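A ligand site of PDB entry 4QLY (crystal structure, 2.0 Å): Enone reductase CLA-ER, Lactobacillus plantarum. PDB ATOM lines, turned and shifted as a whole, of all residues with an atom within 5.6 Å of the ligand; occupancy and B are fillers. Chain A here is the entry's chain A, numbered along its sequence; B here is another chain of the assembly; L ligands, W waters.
O1 of the ligand lies within hydrogen-bond range of NE of Arg 26 (2.7 Å). The backbone NH (N) of Ser 24 lies within hydrogen-bond range of an oxygen (O7) of the ligand (2.7 Å). The side-chain hydroxyl of Ser 24 lies within hydrogen-bond range of an oxygen (O9) of the ligand (2.8 Å). The side-chain amide oxygen (OD1) of Asn 80 sits at hydrogen-bond distance from a nitrogen (N2) of the ligand, 2.8 Å away. NH2 of Arg 208 lies within salt-bridge range of O8 of the ligand (2.8 Å). NH1 of Arg 22 is in salt-bridge range of O9 of the ligand (2.8 Å). N of Gly 171 lies within hydrogen-bond range of O2 of the ligand (3.0 Å). The backbone NH of Ser 170 is in hydrogen-bond range of a nitrogen (N3) of the ligand, 3.0 Å away. N of Ser 51 of chain B sits close to O4 of the ligand, 3.5 Å away. The side-chain hydroxyl (OG1) of Thr 206 sits at hydrogen-bond distance from an oxygen (O8) of the ligand, at 3.4 Å. The side-chain amide nitrogen (NE2) of Gln 83 sits at hydrogen-bond distance from an oxygen (O1) of the ligand, at 3.4 Å.
The side-chain amide nitrogen (ND2) of Asn 167 is in hydrogen-bond range of the side-chain hydroxyl (OG) of Ser 24 (3.2 Å). ND2 of Asn 80 lies within hydrogen-bond range of O of Gly 171, at 3.1 Å. The side-chain amide oxygen of Asn 80 lies within hydrogen-bond range of the side-chain amide nitrogen of Gln 83 (3.1 Å). The guanidinium group (NH1) of Arg 208 lies within hydrogen-bond range of the side-chain hydroxyl (OG1) of Thr 206 (2.9 Å). NH1 of Arg 208 lies within hydrogen-bond range of OD1 of Asn 54 of chain B, 3.1 Å away. NH2 of Arg 208 lies within hydrogen-bond range of O of Ala 49 of chain B, at 3.2 Å. The guanidinium group (NH2) of Arg 22 lies within hydrogen-bond range of the backbone carbonyl oxygen (O) of Thr 48 of chain B (2.9 Å). NE2 of Gln 83 lies within hydrogen-bond range of OD1 of Asn 167 (3.2 Å).
A nitrogen (N4) of the ligand lies close to the backbone carbonyl oxygen of Ala 168 (2.8 Å). His 23 touches the ligand. Phe 79 touches the ligand (CE2 to N2, 3.5 Å). ND2 of Asn 167 touches C13 of the ligand, 3.5 Å away. CA of Phe 169 touches N3 of the ligand (3.0 Å). Pro 50 of chain B touches the ligand (CB to O4, 3.1 Å). Ala 52 of chain B touches the ligand. CB of Asn 54 of chain B touches O5 of the ligand, at 3.4 Å. Ile 146 of chain B touches the ligand (CG2 to C7, 3.5 Å). Of the 28 residues printed, 19 come within 4 Å of the ligand. The nearest printed residue that does not touch the ligand is Cys 53 of chain B (4.1 Å).
Water W5 lies within hydrogen-bond range of an oxygen (O8) of the ligand (2.5 Å), a ring nitrogen (ND1) of His 23 (2.7 Å) and the backbone carbonyl oxygen of Arg 22 (2.8 Å). Water W4 lies within hydrogen-bond range of O7 of the ligand (2.7 Å), O of Leu 204 (2.7 Å) and NH1 of Arg 26 (3.2 Å). Water W1 lies within hydrogen-bond range of an oxygen (O7) of the ligand (2.7 Å), the backbone carbonyl oxygen (O) of Leu 204 (3.0 Å), the side-chain hydroxyl (OG1) of Thr 206 (3.0 Å) and a ring nitrogen (ND1) of His 23 (3.1 Å). Water W6 bridges O3 of the ligand (2.8 Å) and N of Cys 53 of chain B (2.9 Å). Water W2 lies within hydrogen-bond range of an oxygen (O5) of the ligand (2.8 Å) and the guanidinium group (NH2) of Arg 26 (2.9 Å).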
ATOM      1  N   ARG A  22     -26.138  18.371  16.641  1.00  0.00           N
ATOM      2  CA  ARG A  22     -25.398  17.927  17.823  1.00  0.00           C
ATOM      3  C   ARG A  22     -26.110  18.366  19.092  1.00  0.00           C
ATOM      4  O   ARG A  22     -26.377  19.552  19.288  1.00  0.00           O
ATOM      5  CB  ARG A  22     -23.962  18.476  17.814  1.00  0.00           C
ATOM      6  CG  ARG A  22     -23.167  18.049  19.029  1.00  0.00           C
ATOM      7  CD  ARG A  22     -22.236  19.148  19.532  1.00  0.00           C
ATOM      8  NE  ARG A  22     -22.945  20.385  19.851  1.00  0.00           N
ATOM      9  CZ  ARG A  22     -23.655  20.609  20.956  1.00  0.00           C
ATOM     10  NH1 ARG A  22     -23.781  19.651  21.882  1.00  0.00           N
ATOM     11  NH2 ARG A  22     -24.242  21.780  21.135  1.00  0.00           N
ATOM     12  N   HIS A  23     -26.438  17.407  19.958  1.00  0.00           N
ATOM     13  CA  HIS A  23     -26.910  17.743  21.307  1.00  0.00           C
ATOM     14  C   HIS A  23     -26.101  16.957  22.335  1.00  0.00           C
ATOM     15  O   HIS A  23     -25.397  16.011  21.986  1.00  0.00           O
ATOM     16  CB  HIS A  23     -28.408  17.425  21.484  1.00  0.00           C
ATOM     17  CG  HIS A  23     -29.226  17.765  20.283  1.00  0.00           C
ATOM     18  ND1 HIS A  23     -29.694  19.044  20.046  1.00  0.00           N
ATOM     19  CD2 HIS A  23     -29.654  17.013  19.249  1.00  0.00           C
ATOM     20  CE1 HIS A  23     -30.375  19.050  18.913  1.00  0.00           C
ATOM     21  NE2 HIS A  23     -30.351  17.829  18.401  1.00  0.00           N
ATOM     22  N   SER A  24     -26.177  17.380  23.588  1.00  0.00           N
ATOM     23  CA  SER A  24     -25.586  16.613  24.663  1.00  0.00           C
ATOM     24  C   SER A  24     -26.432  15.379  24.941  1.00  0.00           C
ATOM     25  O   SER A  24     -27.551  15.469  25.491  1.00  0.00           O
ATOM     26  CB  SER A  24     -25.446  17.466  25.926  1.00  0.00           C
ATOM     27  OG  SER A  24     -24.407  18.413  25.756  1.00  0.00           O
ATOM     28  N   ARG A  26     -26.844  12.095  27.141  1.00  0.00           N
ATOM     29  CA  ARG A  26     -26.370  11.816  28.489  1.00  0.00           C
ATOM     30  C   ARG A  26     -26.704  10.393  28.924  1.00  0.00           C
ATOM     31  O   ARG A  26     -26.322   9.953  30.007  1.00  0.00           O
ATOM     32  CB  ARG A  26     -26.943  12.823  29.476  1.00  0.00           C
ATOM     33  CG  ARG A  26     -26.517  14.268  29.217  1.00  0.00           C
ATOM     34  CD  ARG A  26     -27.065  15.218  30.288  1.00  0.00           C
ATOM     35  NE  ARG A  26     -26.527  16.566  30.119  1.00  0.00           N
ATOM     36  CZ  ARG A  26     -27.068  17.513  29.359  1.00  0.00           C
ATOM     37  NH1 ARG A  26     -28.184  17.271  28.691  1.00  0.00           N
ATOM     38  NH2 ARG A  26     -26.489  18.710  29.257  1.00  0.00           N
ATOM     39  N   PHE A  79     -24.143  13.998  39.778  1.00  0.00           N
ATOM     40  CA  PHE A  79     -25.172  14.297  38.776  1.00  0.00           C
ATOM     41  C   PHE A  79     -24.687  13.984  37.345  1.00  0.00           C
ATOM     42  O   PHE A  79     -25.487  13.879  36.431  1.00  0.00           O
ATOM     43  CB  PHE A  79     -25.653  15.744  38.892  1.00  0.00           C
ATOM     44  CG  PHE A  79     -24.791  16.753  38.185  1.00  0.00           C
ATOM     45  CD1 PHE A  79     -23.687  17.307  38.818  1.00  0.00           C
ATOM     46  CD2 PHE A  79     -25.112  17.181  36.902  1.00  0.00           C
ATOM     47  CE1 PHE A  79     -22.909  18.239  38.171  1.00  0.00           C
ATOM     48  CE2 PHE A  79     -24.336  18.124  36.264  1.00  0.00           C
ATOM     49  CZ  PHE A  79     -23.222  18.656  36.891  1.00  0.00           C
ATOM     50  N   ASN A  80     -23.372  13.809  37.172  1.00  0.00           N
ATOM     51  CA  ASN A  80     -22.787  13.355  35.904  1.00  0.00           C
ATOM     52  C   ASN A  80     -22.494  11.853  35.851  1.00  0.00           C
ATOM     53  O   ASN A  80     -21.859  11.367  34.899  1.00  0.00           O
ATOM     54  CB  ASN A  80     -21.505  14.144  35.615  1.00  0.00           C
ATOM     55  CG  ASN A  80     -21.783  15.591  35.232  1.00  0.00           C
ATOM     56  OD1 ASN A  80     -22.818  15.889  34.612  1.00  0.00           O
ATOM     57  ND2 ASN A  80     -20.876  16.492  35.594  1.00  0.00           N
ATOM     58  N   GLN A  83     -23.911   9.720  32.588  1.00  0.00           N
ATOM     59  CA  GLN A  83     -23.090   9.728  31.384  1.00  0.00           C
ATOM     60  C   GLN A  83     -21.911   8.808  31.575  1.00  0.00           C
ATOM     61  O   GLN A  83     -21.620   7.994  30.705  1.00  0.00           O
ATOM     62  CB  GLN A  83     -22.580  11.137  31.025  1.00  0.00           C
ATOM     63  CG  GLN A  83     -23.630  12.197  30.873  1.00  0.00           C
ATOM     64  CD  GLN A  83     -23.981  12.869  32.198  1.00  0.00           C
ATOM     65  OE1 GLN A  83     -24.423  12.212  33.138  1.00  0.00           O
ATOM     66  NE2 GLN A  83     -23.793  14.194  32.254  1.00  0.00           N
ATOM     67  N   ASN A 167     -21.246  13.899  25.234  1.00  0.00           N
ATOM     68  CA  ASN A 167     -21.545  14.952  26.181  1.00  0.00           C
ATOM     69  C   ASN A 167     -20.270  15.484  26.786  1.00  0.00           C
ATOM     70  O   ASN A 167     -19.467  14.713  27.324  1.00  0.00           O
ATOM     71  CB  ASN A 167     -22.468  14.453  27.276  1.00  0.00           C
ATOM     72  CG  ASN A 167     -22.591  15.458  28.406  1.00  0.00           C
ATOM     73  OD1 ASN A 167     -22.330  15.150  29.569  1.00  0.00           O
ATOM     74  ND2 ASN A 167     -22.939  16.705  28.057  1.00  0.00           N
ATOM     75  N   ALA A 168     -20.077  16.807  26.699  1.00  0.00           N
ATOM     76  CA  ALA A 168     -18.980  17.468  27.402  1.00  0.00           C
ATOM     77  C   ALA A 168     -19.437  17.796  28.808  1.00  0.00           C
ATOM     78  O   ALA A 168     -20.577  18.236  29.007  1.00  0.00           O
ATOM     79  CB  ALA A 168     -18.532  18.735  26.669  1.00  0.00           C
ATOM     80  N   PHE A 169     -18.565  17.614  29.779  1.00  0.00           N
ATOM     81  CA  PHE A 169     -18.926  17.968  31.144  1.00  0.00           C
ATOM     82  C   PHE A 169     -17.735  18.424  31.964  1.00  0.00           C
ATOM     83  O   PHE A 169     -16.612  17.947  31.775  1.00  0.00           O
ATOM     84  CB  PHE A 169     -19.644  16.789  31.831  1.00  0.00           C
ATOM     85  CG  PHE A 169     -18.797  15.551  31.982  1.00  0.00           C
ATOM     86  CD1 PHE A 169     -18.731  14.601  30.967  1.00  0.00           C
ATOM     87  CD2 PHE A 169     -18.073  15.330  33.149  1.00  0.00           C
ATOM     88  CE1 PHE A 169     -17.957  13.452  31.112  1.00  0.00           C
ATOM     89  CE2 PHE A 169     -17.289  14.180  33.296  1.00  0.00           C
ATOM     90  CZ  PHE A 169     -17.241  13.242  32.275  1.00  0.00           C
ATOM     91  N   SER A 170     -17.972  19.367  32.875  1.00  0.00           N
ATOM     92  CA  SER A 170     -16.917  19.874  33.759  1.00  0.00           C
ATOM     93  C   SER A 170     -17.439  19.897  35.180  1.00  0.00           C
ATOM     94  O   SER A 170     -16.841  20.508  36.065  1.00  0.00           O
ATOM     95  CB  SER A 170     -16.438  21.280  33.321  1.00  0.00           C
ATOM     96  OG  SER A 170     -17.492  22.221  33.335  1.00  0.00           O
ATOM     97  N   GLY A 171     -18.548  19.214  35.399  1.00  0.00           N
ATOM     98  CA  GLY A 171     -19.112  19.095  36.730  1.00  0.00           C
ATOM     99  C   GLY A 171     -18.244  18.122  37.502  1.00  0.00           C
ATOM    100  O   GLY A 171     -18.596  16.953  37.658  1.00  0.00           O
ATOM    101  N   MET A 192     -12.258  19.431  30.709  1.00  0.00           N
ATOM    102  CA  MET A 192     -13.577  18.824  30.525  1.00  0.00           C
ATOM    103  C   MET A 192     -13.487  17.348  30.222  1.00  0.00           C
ATOM    104  O   MET A 192     -12.454  16.849  29.733  1.00  0.00           O
ATOM    105  CB  MET A 192     -14.334  19.526  29.385  1.00  0.00           C
ATOM    106  CG  MET A 192     -13.793  19.211  28.019  1.00  0.00           C
ATOM    107  SD  MET A 192     -14.604  20.106  26.679  1.00  0.00           S
ATOM    108  CE  MET A 192     -14.101  21.795  26.974  1.00  0.00           C
ATOM    109  N   PRO A 203     -31.882  13.346  23.666  1.00  0.00           N
ATOM    110  CA  PRO A 203     -31.224  14.379  24.481  1.00  0.00           C
ATOM    111  C   PRO A 203     -32.196  15.508  24.848  1.00  0.00           C
ATOM    112  O   PRO A 203     -33.109  15.810  24.082  1.00  0.00           O
ATOM    113  CB  PRO A 203     -30.100  14.878  23.571  1.00  0.00           C
ATOM    114  CG  PRO A 203     -30.577  14.600  22.186  1.00  0.00           C
ATOM    115  CD  PRO A 203     -31.424  13.362  22.267  1.00  0.00           C
ATOM    116  N   LEU A 204     -32.001  16.087  26.039  1.00  0.00           N
ATOM    117  CA  LEU A 204     -32.773  17.257  26.452  1.00  0.00           C
ATOM    118  C   LEU A 204     -32.673  18.359  25.401  1.00  0.00           C
ATOM    119  O   LEU A 204     -31.569  18.692  24.948  1.00  0.00           O
ATOM    120  CB  LEU A 204     -32.274  17.782  27.807  1.00  0.00           C
ATOM    121  CG  LEU A 204     -32.701  17.090  29.117  1.00  0.00           C
ATOM    122  CD1 LEU A 204     -32.310  15.623  29.137  1.00  0.00           C
ATOM    123  CD2 LEU A 204     -32.137  17.810  30.334  1.00  0.00           C
ATOM    124  N   THR A 206     -32.596  22.060  23.810  1.00  0.00           N
ATOM    125  CA  THR A 206     -32.182  23.388  24.274  1.00  0.00           C
ATOM    126  C   THR A 206     -32.411  24.435  23.188  1.00  0.00           C
ATOM    127  O   THR A 206     -32.610  24.129  22.000  1.00  0.00           O
ATOM    128  CB  THR A 206     -30.670  23.446  24.707  1.00  0.00           C
ATOM    129  OG1 THR A 206     -29.818  23.094  23.609  1.00  0.00           O
ATOM    130  CG2 THR A 206     -30.373  22.509  25.892  1.00  0.00           C
ATOM    131  N   ARG A 208     -30.983  28.540  21.820  1.00  0.00           N
ATOM    132  CA  ARG A 208     -29.923  29.513  21.902  1.00  0.00           C
ATOM    133  C   ARG A 208     -30.532  30.912  21.855  1.00  0.00           C
ATOM    134  O   ARG A 208     -31.605  31.095  21.259  1.00  0.00           O
ATOM    135  CB  ARG A 208     -28.918  29.342  20.761  1.00  0.00           C
ATOM    136  CG  ARG A 208     -28.200  27.995  20.726  1.00  0.00           C
ATOM    137  CD  ARG A 208     -27.224  27.833  21.866  1.00  0.00           C
ATOM    138  NE  ARG A 208     -26.517  26.551  21.738  1.00  0.00           N
ATOM    139  CZ  ARG A 208     -26.985  25.386  22.185  1.00  0.00           C
ATOM    140  NH1 ARG A 208     -28.145  25.326  22.835  1.00  0.00           N
ATOM    141  NH2 ARG A 208     -26.285  24.291  21.995  1.00  0.00           N
ATOM    142  N   THR B  48     -24.353  27.306  17.715  1.00  0.00           N
ATOM    143  CA  THR B  48     -24.998  26.025  18.079  1.00  0.00           C
ATOM    144  C   THR B  48     -24.119  25.246  19.041  1.00  0.00           C
ATOM    145  O   THR B  48     -24.538  24.215  19.590  1.00  0.00           O
ATOM    146  CB  THR B  48     -25.267  25.130  16.861  1.00  0.00           C
ATOM    147  OG1 THR B  48     -24.058  24.935  16.126  1.00  0.00           O
ATOM    148  CG2 THR B  48     -26.316  25.791  15.952  1.00  0.00           C
ATOM    149  N   ALA B  49     -22.907  25.756  19.239  1.00  0.00           N
ATOM    150  CA  ALA B  49     -21.923  25.163  20.145  1.00  0.00           C
ATOM    151  C   ALA B  49     -22.502  24.938  21.536  1.00  0.00           C
ATOM    152  O   ALA B  49     -23.428  25.661  21.936  1.00  0.00           O
ATOM    153  CB  ALA B  49     -20.672  26.062  20.220  1.00  0.00           C
ATOM    154  N   PRO B  50     -21.967  23.940  22.258  1.00  0.00           N
ATOM    155  CA  PRO B  50     -22.359  23.703  23.644  1.00  0.00           C
ATOM    156  C   PRO B  50     -21.748  24.731  24.593  1.00  0.00           C
ATOM    157  O   PRO B  50     -20.854  25.486  24.190  1.00  0.00           O
ATOM    158  CB  PRO B  50     -21.804  22.297  23.937  1.00  0.00           C
ATOM    159  CG  PRO B  50     -20.602  22.184  23.057  1.00  0.00           C
ATOM    160  CD  PRO B  50     -20.878  23.025  21.836  1.00  0.00           C
ATOM    161  N   SER B  51     -22.230  24.766  25.826  1.00  0.00           N
ATOM    162  CA  SER B  51     -21.709  25.668  26.837  1.00  0.00           C
ATOM    163  C   SER B  51     -22.210  25.189  28.190  1.00  0.00           C
ATOM    164  O   SER B  51     -23.312  24.658  28.281  1.00  0.00           O
ATOM    165  CB  SER B  51     -22.120  27.119  26.566  1.00  0.00           C
ATOM    166  OG  SER B  51     -23.538  27.241  26.521  1.00  0.00           O
ATOM    167  N   ALA B  52     -21.414  25.385  29.238  1.00  0.00           N
ATOM    168  CA  ALA B  52     -21.841  24.957  30.564  1.00  0.00           C
ATOM    169  C   ALA B  52     -23.133  25.669  30.935  1.00  0.00           C
ATOM    170  O   ALA B  52     -23.242  26.891  30.773  1.00  0.00           O
ATOM    171  CB  ALA B  52     -20.743  25.228  31.596  1.00  0.00           C
ATOM    172  N   CYS B  53     -24.108  24.878  31.395  1.00  0.00           N
ATOM    173  CA  CYS B  53     -25.456  25.344  31.767  1.00  0.00           C
ATOM    174  C   CYS B  53     -26.128  26.149  30.658  1.00  0.00           C
ATOM    175  O   CYS B  53     -27.001  26.956  30.927  1.00  0.00           O
ATOM    176  CB  CYS B  53     -25.397  26.178  33.053  1.00  0.00           C
ATOM    177  SG  CYS B  53     -24.877  25.227  34.533  1.00  0.00           S
ATOM    178  N   ASN B  54     -25.737  25.891  29.414  1.00  0.00           N
ATOM    179  CA  ASN B  54     -26.225  26.640  28.253  1.00  0.00           C
ATOM    180  C   ASN B  54     -26.208  28.166  28.443  1.00  0.00           C
ATOM    181  O   ASN B  54     -27.107  28.872  27.971  1.00  0.00           O
ATOM    182  CB  ASN B  54     -27.642  26.163  27.897  1.00  0.00           C
ATOM    183  CG  ASN B  54     -28.028  26.549  26.488  1.00  0.00           C
ATOM    184  OD1 ASN B  54     -27.183  26.526  25.582  1.00  0.00           O
ATOM    185  ND2 ASN B  54     -29.288  26.934  26.290  1.00  0.00           N
ATOM    186  N   ASP B 143     -14.638  29.476  32.735  1.00  0.00           N
ATOM    187  CA  ASP B 143     -15.811  28.937  32.053  1.00  0.00           C
ATOM    188  C   ASP B 143     -16.154  29.722  30.789  1.00  0.00           C
ATOM    189  O   ASP B 143     -16.530  29.126  29.773  1.00  0.00           O
ATOM    190  CB  ASP B 143     -17.014  28.925  33.007  1.00  0.00           C
ATOM    191  CG  ASP B 143     -18.187  28.131  32.433  1.00  0.00           C
ATOM    192  OD1 ASP B 143     -18.050  26.903  32.283  1.00  0.00           O
ATOM    193  OD2 ASP B 143     -19.248  28.738  32.149  1.00  0.00           O
ATOM    194  N   ILE B 146     -13.707  28.894  27.921  1.00  0.00           N
ATOM    195  CA  ILE B 146     -14.076  27.621  27.307  1.00  0.00           C
ATOM    196  C   ILE B 146     -15.202  27.800  26.314  1.00  0.00           C
ATOM    197  O   ILE B 146     -15.137  27.296  25.191  1.00  0.00           O
ATOM    198  CB  ILE B 146     -14.498  26.557  28.377  1.00  0.00           C
ATOM    199  CG1 ILE B 146     -13.298  26.147  29.235  1.00  0.00           C
ATOM    200  CG2 ILE B 146     -15.075  25.343  27.705  1.00  0.00           C
ATOM    201  CD1 ILE B 146     -13.679  25.196  30.387  1.00  0.00           C
ATOM    202  N   ASP B 147     -16.235  28.526  26.728  1.00  0.00           N
ATOM    203  CA  ASP B 147     -17.338  28.832  25.852  1.00  0.00           C
ATOM    204  C   ASP B 147     -16.866  29.573  24.589  1.00  0.00           C
ATOM    205  O   ASP B 147     -17.235  29.212  23.478  1.00  0.00           O
ATOM    206  CB  ASP B 147     -18.369  29.693  26.595  1.00  0.00           C
ATOM    207  CG  ASP B 147     -19.242  28.884  27.537  1.00  0.00           C
ATOM    208  OD1 ASP B 147     -19.023  27.647  27.666  1.00  0.00           O
ATOM    209  OD2 ASP B 147     -20.144  29.507  28.129  1.00  0.00           O
ATOM    210  N   VAL B 150     -14.975  27.030  22.224  1.00  0.00           N
ATOM    211  CA  VAL B 150     -15.723  26.041  21.455  1.00  0.00           C
ATOM    212  C   VAL B 150     -16.531  26.741  20.353  1.00  0.00           C
ATOM    213  O   VAL B 150     -16.650  26.210  19.249  1.00  0.00           O
ATOM    214  CB  VAL B 150     -16.647  25.145  22.362  1.00  0.00           C
ATOM    215  CG1 VAL B 150     -15.805  24.324  23.370  1.00  0.00           C
ATOM    216  CG2 VAL B 150     -17.749  25.951  23.072  1.00  0.00           C
HETATM  217  N1  LIG L   1     -23.680  18.831  30.835  1.00  0.00           N
HETATM  218  C1  LIG L   1     -23.915  18.105  31.990  1.00  0.00           C
HETATM  219  O1  LIG L   1     -24.908  17.399  32.073  1.00  0.00           O
HETATM  220  N2  LIG L   1     -23.046  18.153  33.061  1.00  0.00           N
HETATM  221  C2  LIG L   1     -21.910  18.933  32.974  1.00  0.00           C
HETATM  222  O2  LIG L   1     -21.116  18.982  33.933  1.00  0.00           O
HETATM  223  C3  LIG L   1     -21.673  19.658  31.809  1.00  0.00           C
HETATM  224  N3  LIG L   1     -20.547  20.439  31.720  1.00  0.00           N
HETATM  225  C4  LIG L   1     -20.283  21.142  30.565  1.00  0.00           C
HETATM  226  C5  LIG L   1     -19.119  21.891  30.519  1.00  0.00           C
HETATM  227  C6  LIG L   1     -18.807  22.610  29.384  1.00  0.00           C
HETATM  228  C7  LIG L   1     -17.554  23.430  29.343  1.00  0.00           C
HETATM  229  C8  LIG L   1     -19.656  22.578  28.285  1.00  0.00           C
HETATM  230  C9  LIG L   1     -19.295  23.375  27.072  1.00  0.00           C
HETATM  231  C10 LIG L   1     -20.833  21.820  28.339  1.00  0.00           C
HETATM  232  C11 LIG L   1     -21.158  21.094  29.482  1.00  0.00           C
HETATM  233  N4  LIG L   1     -22.316  20.316  29.573  1.00  0.00           N
HETATM  234  C12 LIG L   1     -22.562  19.602  30.734  1.00  0.00           C
HETATM  235  C13 LIG L   1     -23.332  20.211  28.450  1.00  0.00           C
HETATM  236  C14 LIG L   1     -24.232  21.483  28.396  1.00  0.00           C
HETATM  237  O3  LIG L   1     -25.212  21.510  29.423  1.00  0.00           O
HETATM  238  C15 LIG L   1     -24.974  21.644  27.077  1.00  0.00           C
HETATM  239  O4  LIG L   1     -24.004  21.770  26.063  1.00  0.00           O
HETATM  240  C16 LIG L   1     -25.890  22.885  26.991  1.00  0.00           C
HETATM  241  O5  LIG L   1     -27.003  22.795  27.852  1.00  0.00           O
HETATM  242  C17 LIG L   1     -26.399  23.001  25.558  1.00  0.00           C
HETATM  243  O6  LIG L   1     -27.080  21.806  25.251  1.00  0.00           O
HETATM  244  P1  LIG L   1     -26.692  20.911  23.979  1.00  0.00           P
HETATM  245  O7  LIG L   1     -27.533  19.657  23.991  1.00  0.00           O
HETATM  246  O8  LIG L   1     -26.896  21.657  22.682  1.00  0.00           O
HETATM  247  O9  LIG L   1     -25.234  20.499  24.125  1.00  0.00           O
HETATM  248  O   HOH W   1     -30.002  20.146  22.891  1.00  0.00           O
HETATM  249  O   HOH W   2     -28.503  20.403  28.095  1.00  0.00           O
HETATM  250  O   HOH W   3     -26.116  15.501  33.861  1.00  0.00           O
HETATM  251  O   HOH W   4     -29.088  18.899  26.063  1.00  0.00           O
HETATM  252  O   HOH W   5     -28.182  21.241  20.602  1.00  0.00           O
HETATM  253  O   HOH W   6     -24.104  22.056  31.881  1.00  0.00           O
